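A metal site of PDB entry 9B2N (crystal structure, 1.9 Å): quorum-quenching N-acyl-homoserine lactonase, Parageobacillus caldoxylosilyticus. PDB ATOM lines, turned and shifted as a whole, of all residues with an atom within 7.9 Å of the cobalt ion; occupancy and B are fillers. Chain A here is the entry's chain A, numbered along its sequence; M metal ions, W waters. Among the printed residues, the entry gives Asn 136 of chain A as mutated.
The cobalt ion is bound by the side-chain carboxylate (OD2) of Asp 234 (2.2 Å), a ring nitrogen (NE2) of His 212 (2.2 Å), a ring nitrogen (NE2) of His 132 (2.2 Å), a ring nitrogen (ND1) of His 134 (2.2 Å), water W2 (2.2 Å) and water W1 (2.4 Å).
Four residues have an atom within 4 Å of the cobalt ion: His 132, His 134, His 212 and Asp 234.
The side-chain carboxylate (OD1) of Asp 234 lies within hydrogen-bond range of a ring nitrogen (NE2) of His 137 (3.2 Å). A ring nitrogen (ND1) of His 212 lies within hydrogen-bond range of the backbone carbonyl oxygen (O) of Ile 251 (3.0 Å). The side-chain hydroxyl (OG) of Ser 131 is in hydrogen-bond range of a ring nitrogen (ND1) of His 132, 3.0 Å away. The side-chain hydroxyl of Tyr 172 is in hydrogen-bond range of a ring nitrogen (NE2) of His 134.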
ATOM      1  N   SER A 131      -4.930  16.405 -24.862  1.00  0.00           N
ATOM      2  CA  SER A 131      -5.799  16.673 -23.727  1.00  0.00           C
ATOM      3  C   SER A 131      -6.836  15.572 -23.612  1.00  0.00           C
ATOM      4  O   SER A 131      -7.193  15.143 -22.511  1.00  0.00           O
ATOM      5  CB  SER A 131      -6.449  18.045 -23.837  1.00  0.00           C
ATOM      6  OG  SER A 131      -7.345  18.090 -24.939  1.00  0.00           O
ATOM      7  N   HIS A 132      -7.322  15.133 -24.773  1.00  0.00           N
ATOM      8  CA  HIS A 132      -8.223  13.997 -24.922  1.00  0.00           C
ATOM      9  C   HIS A 132      -8.339  13.733 -26.423  1.00  0.00           C
ATOM     10  O   HIS A 132      -7.739  14.446 -27.218  1.00  0.00           O
ATOM     11  CB  HIS A 132      -9.523  14.213 -24.146  1.00  0.00           C
ATOM     12  CG  HIS A 132     -10.398  15.316 -24.654  1.00  0.00           C
ATOM     13  ND1 HIS A 132      -9.986  16.628 -24.809  1.00  0.00           N
ATOM     14  CD2 HIS A 132     -11.694  15.304 -24.999  1.00  0.00           C
ATOM     15  CE1 HIS A 132     -11.005  17.365 -25.252  1.00  0.00           C
ATOM     16  NE2 HIS A 132     -12.050  16.577 -25.380  1.00  0.00           N
ATOM     17  N   LEU A 133      -9.106  12.710 -26.817  1.00  0.00           N
ATOM     18  CA  LEU A 133      -9.059  12.218 -28.188  1.00  0.00           C
ATOM     19  C   LEU A 133     -10.353  12.531 -28.929  1.00  0.00           C
ATOM     20  O   LEU A 133     -10.734  11.804 -29.845  1.00  0.00           O
ATOM     21  CB  LEU A 133      -8.742  10.719 -28.179  1.00  0.00           C
ATOM     22  CG  LEU A 133      -7.360  10.338 -27.633  1.00  0.00           C
ATOM     23  CD1 LEU A 133      -7.117   8.846 -27.711  1.00  0.00           C
ATOM     24  CD2 LEU A 133      -6.265  11.104 -28.363  1.00  0.00           C
ATOM     25  N   HIS A 134     -11.011  13.640 -28.548  1.00  0.00           N
ATOM     26  CA  HIS A 134     -12.201  14.103 -29.240  1.00  0.00           C
ATOM     27  C   HIS A 134     -11.826  14.664 -30.613  1.00  0.00           C
ATOM     28  O   HIS A 134     -10.671  14.999 -30.856  1.00  0.00           O
ATOM     29  CB  HIS A 134     -12.959  15.142 -28.396  1.00  0.00           C
ATOM     30  CG  HIS A 134     -13.941  14.551 -27.440  1.00  0.00           C
ATOM     31  ND1 HIS A 134     -14.578  15.292 -26.459  1.00  0.00           N
ATOM     32  CD2 HIS A 134     -14.416  13.306 -27.321  1.00  0.00           C
ATOM     33  CE1 HIS A 134     -15.405  14.499 -25.780  1.00  0.00           C
ATOM     34  NE2 HIS A 134     -15.323  13.288 -26.287  1.00  0.00           N
ATOM     35  N   LEU A 135     -12.832  14.792 -31.479  1.00  0.00           N
ATOM     36  CA  LEU A 135     -12.643  15.094 -32.899  1.00  0.00           C
ATOM     37  C   LEU A 135     -11.891  16.415 -33.086  1.00  0.00           C
ATOM     38  O   LEU A 135     -11.147  16.554 -34.058  1.00  0.00           O
ATOM     39  CB  LEU A 135     -14.005  15.108 -33.598  1.00  0.00           C
ATOM     40  CG  LEU A 135     -14.960  16.242 -33.236  1.00  0.00           C
ATOM     41  CD1 LEU A 135     -16.233  16.151 -34.075  1.00  0.00           C
ATOM     42  CD2 LEU A 135     -15.303  16.262 -31.749  1.00  0.00           C
ATOM     43  N   ASN A 136     -12.092  17.376 -32.173  1.00  0.00           N
ATOM     44  CA  ASN A 136     -11.563  18.715 -32.346  1.00  0.00           C
ATOM     45  C   ASN A 136     -10.304  18.920 -31.507  1.00  0.00           C
ATOM     46  O   ASN A 136      -9.902  20.066 -31.274  1.00  0.00           O
ATOM     47  CB  ASN A 136     -12.609  19.788 -32.048  1.00  0.00           C
ATOM     48  CG  ASN A 136     -13.287  19.580 -30.707  1.00  0.00           C
ATOM     49  OD1 ASN A 136     -13.074  18.556 -30.049  1.00  0.00           O
ATOM     50  ND2 ASN A 136     -14.118  20.524 -30.294  1.00  0.00           N
ATOM     51  N   HIS A 137      -9.665  17.829 -31.070  1.00  0.00           N
ATOM     52  CA  HIS A 137      -8.450  17.936 -30.281  1.00  0.00           C
ATOM     53  C   HIS A 137      -7.364  16.997 -30.817  1.00  0.00           C
ATOM     54  O   HIS A 137      -6.183  17.296 -30.707  1.00  0.00           O
ATOM     55  CB  HIS A 137      -8.731  17.693 -28.785  1.00  0.00           C
ATOM     56  CG  HIS A 137      -9.565  18.768 -28.150  1.00  0.00           C
ATOM     57  ND1 HIS A 137      -9.030  19.798 -27.411  1.00  0.00           N
ATOM     58  CD2 HIS A 137     -10.887  18.961 -28.154  1.00  0.00           C
ATOM     59  CE1 HIS A 137     -10.002  20.590 -26.982  1.00  0.00           C
ATOM     60  NE2 HIS A 137     -11.140  20.099 -27.425  1.00  0.00           N
ATOM     61  N   GLU A 155      -8.274   7.364 -21.823  1.00  0.00           N
ATOM     62  CA  GLU A 155      -8.781   8.009 -23.030  1.00  0.00           C
ATOM     63  C   GLU A 155      -8.370   7.187 -24.250  1.00  0.00           C
ATOM     64  O   GLU A 155      -9.181   6.991 -25.162  1.00  0.00           O
ATOM     65  CB  GLU A 155      -8.245   9.440 -23.131  1.00  0.00           C
ATOM     66  CG  GLU A 155      -8.852  10.253 -24.264  1.00  0.00           C
ATOM     67  CD  GLU A 155     -10.305  10.653 -24.056  1.00  0.00           C
ATOM     68  OE1 GLU A 155     -10.840  10.361 -22.969  1.00  0.00           O
ATOM     69  OE2 GLU A 155     -10.901  11.245 -24.982  1.00  0.00           O
ATOM     70  N   ALA A 171     -17.998  11.437 -31.086  1.00  0.00           N
ATOM     71  CA  ALA A 171     -16.964  12.460 -30.989  1.00  0.00           C
ATOM     72  C   ALA A 171     -15.582  11.855 -31.228  1.00  0.00           C
ATOM     73  O   ALA A 171     -14.584  12.575 -31.200  1.00  0.00           O
ATOM     74  CB  ALA A 171     -17.053  13.137 -29.646  1.00  0.00           C
ATOM     75  N   TYR A 172     -15.528  10.540 -31.450  1.00  0.00           N
ATOM     76  CA  TYR A 172     -14.277   9.851 -31.735  1.00  0.00           C
ATOM     77  C   TYR A 172     -14.289   9.399 -33.193  1.00  0.00           C
ATOM     78  O   TYR A 172     -15.121   8.579 -33.586  1.00  0.00           O
ATOM     79  CB  TYR A 172     -14.090   8.702 -30.730  1.00  0.00           C
ATOM     80  CG  TYR A 172     -13.888   9.191 -29.303  1.00  0.00           C
ATOM     81  CD1 TYR A 172     -12.639   9.623 -28.856  1.00  0.00           C
ATOM     82  CD2 TYR A 172     -14.952   9.269 -28.412  1.00  0.00           C
ATOM     83  CE1 TYR A 172     -12.460  10.096 -27.569  1.00  0.00           C
ATOM     84  CE2 TYR A 172     -14.784   9.740 -27.116  1.00  0.00           C
ATOM     85  CZ  TYR A 172     -13.527  10.149 -26.695  1.00  0.00           C
ATOM     86  OH  TYR A 172     -13.361  10.616 -25.423  1.00  0.00           O
ATOM     87  N   HIS A 212     -14.911  15.190 -18.169  1.00  0.00           N
ATOM     88  CA  HIS A 212     -15.462  15.495 -19.480  1.00  0.00           C
ATOM     89  C   HIS A 212     -15.414  14.229 -20.340  1.00  0.00           C
ATOM     90  O   HIS A 212     -16.413  13.855 -20.950  1.00  0.00           O
ATOM     91  CB  HIS A 212     -14.707  16.662 -20.130  1.00  0.00           C
ATOM     92  CG  HIS A 212     -15.010  16.873 -21.575  1.00  0.00           C
ATOM     93  ND1 HIS A 212     -16.238  17.290 -22.036  1.00  0.00           N
ATOM     94  CD2 HIS A 212     -14.243  16.709 -22.668  1.00  0.00           C
ATOM     95  CE1 HIS A 212     -16.206  17.373 -23.362  1.00  0.00           C
ATOM     96  NE2 HIS A 212     -15.006  17.031 -23.766  1.00  0.00           N
ATOM     97  N   ALA A 213     -14.243  13.578 -20.344  1.00  0.00           N
ATOM     98  CA  ALA A 213     -14.039  12.364 -21.114  1.00  0.00           C
ATOM     99  C   ALA A 213     -13.396  11.294 -20.227  1.00  0.00           C
ATOM    100  O   ALA A 213     -13.302  11.471 -19.010  1.00  0.00           O
ATOM    101  CB  ALA A 213     -13.191  12.667 -22.335  1.00  0.00           C
ATOM    102  N   MET A 216      -8.497  13.011 -19.087  1.00  0.00           N
ATOM    103  CA  MET A 216      -8.191  14.397 -19.437  1.00  0.00           C
ATOM    104  C   MET A 216      -6.778  14.746 -18.984  1.00  0.00           C
ATOM    105  O   MET A 216      -6.394  14.472 -17.854  1.00  0.00           O
ATOM    106  CB  MET A 216      -9.190  15.351 -18.777  1.00  0.00           C
ATOM    107  CG  MET A 216     -10.637  15.055 -19.094  1.00  0.00           C
ATOM    108  SD  MET A 216     -11.006  15.216 -20.852  1.00  0.00           S
ATOM    109  CE  MET A 216     -10.787  16.982 -21.106  1.00  0.00           C
ATOM    110  N   SER A 233      -8.059  22.872 -21.439  1.00  0.00           N
ATOM    111  CA  SER A 233      -8.795  22.247 -22.518  1.00  0.00           C
ATOM    112  C   SER A 233     -10.249  22.058 -22.085  1.00  0.00           C
ATOM    113  O   SER A 233     -10.817  22.929 -21.436  1.00  0.00           O
ATOM    114  CB  SER A 233      -8.153  20.953 -22.943  1.00  0.00           C
ATOM    115  OG  SER A 233      -8.893  20.338 -23.993  1.00  0.00           O
ATOM    116  N   ASP A 234     -10.839  20.903 -22.424  1.00  0.00           N
ATOM    117  CA  ASP A 234     -12.267  20.695 -22.245  1.00  0.00           C
ATOM    118  C   ASP A 234     -12.609  20.321 -20.801  1.00  0.00           C
ATOM    119  O   ASP A 234     -13.749  19.973 -20.513  1.00  0.00           O
ATOM    120  CB  ASP A 234     -12.807  19.655 -23.228  1.00  0.00           C
ATOM    121  CG  ASP A 234     -13.004  20.168 -24.653  1.00  0.00           C
ATOM    122  OD1 ASP A 234     -12.732  21.360 -24.890  1.00  0.00           O
ATOM    123  OD2 ASP A 234     -13.442  19.368 -25.505  1.00  0.00           O
ATOM    124  N   ALA A 235     -11.633  20.396 -19.897  1.00  0.00           N
ATOM    125  CA  ALA A 235     -11.920  20.201 -18.483  1.00  0.00           C
ATOM    126  C   ALA A 235     -12.742  21.393 -17.984  1.00  0.00           C
ATOM    127  O   ALA A 235     -13.499  21.279 -17.023  1.00  0.00           O
ATOM    128  CB  ALA A 235     -10.639  20.044 -17.703  1.00  0.00           C
ATOM    129  N   TYR A 237     -14.853  24.318 -20.322  1.00  0.00           N
ATOM    130  CA  TYR A 237     -15.190  24.869 -21.620  1.00  0.00           C
ATOM    131  C   TYR A 237     -14.973  26.384 -21.643  1.00  0.00           C
ATOM    132  O   TYR A 237     -14.276  26.884 -22.520  1.00  0.00           O
ATOM    133  CB  TYR A 237     -16.646  24.503 -21.946  1.00  0.00           C
ATOM    134  CG  TYR A 237     -16.894  23.180 -22.672  1.00  0.00           C
ATOM    135  CD1 TYR A 237     -15.894  22.554 -23.409  1.00  0.00           C
ATOM    136  CD2 TYR A 237     -18.145  22.580 -22.640  1.00  0.00           C
ATOM    137  CE1 TYR A 237     -16.128  21.358 -24.082  1.00  0.00           C
ATOM    138  CE2 TYR A 237     -18.393  21.397 -23.305  1.00  0.00           C
ATOM    139  CZ  TYR A 237     -17.386  20.773 -24.034  1.00  0.00           C
ATOM    140  OH  TYR A 237     -17.632  19.606 -24.694  1.00  0.00           O
ATOM    141  N   ILE A 251     -21.901  17.206 -22.677  1.00  0.00           N
ATOM    142  CA  ILE A 251     -20.878  16.248 -23.065  1.00  0.00           C
ATOM    143  C   ILE A 251     -20.032  15.943 -21.825  1.00  0.00           C
ATOM    144  O   ILE A 251     -19.165  16.723 -21.463  1.00  0.00           O
ATOM    145  CB  ILE A 251     -19.990  16.752 -24.226  1.00  0.00           C
ATOM    146  CG1 ILE A 251     -20.801  17.162 -25.465  1.00  0.00           C
ATOM    147  CG2 ILE A 251     -18.930  15.713 -24.576  1.00  0.00           C
ATOM    148  CD1 ILE A 251     -19.958  17.364 -26.715  1.00  0.00           C
ATOM    149  N   HIS A 280     -12.619  26.596 -24.860  1.00  0.00           N
ATOM    150  CA  HIS A 280     -13.171  27.407 -25.946  1.00  0.00           C
ATOM    151  C   HIS A 280     -14.039  28.540 -25.411  1.00  0.00           C
ATOM    152  O   HIS A 280     -15.263  28.570 -25.571  1.00  0.00           O
ATOM    153  CB  HIS A 280     -13.786  26.517 -27.039  1.00  0.00           C
ATOM    154  CG  HIS A 280     -14.816  25.528 -26.580  1.00  0.00           C
ATOM    155  ND1 HIS A 280     -14.671  24.175 -26.815  1.00  0.00           N
ATOM    156  CD2 HIS A 280     -15.975  25.675 -25.934  1.00  0.00           C
ATOM    157  CE1 HIS A 280     -15.722  23.530 -26.320  1.00  0.00           C
ATOM    158  NE2 HIS A 280     -16.522  24.425 -25.777  1.00  0.00           N
HETATM  159 CO    CO M   1     -14.088  17.312 -25.711  1.00  0.00          CO
HETATM  160  O   HOH W   1     -14.409  18.281 -27.924  1.00  0.00           O
HETATM  161  O   HOH W   2     -16.044  18.319 -26.143  1.00  0.00           O
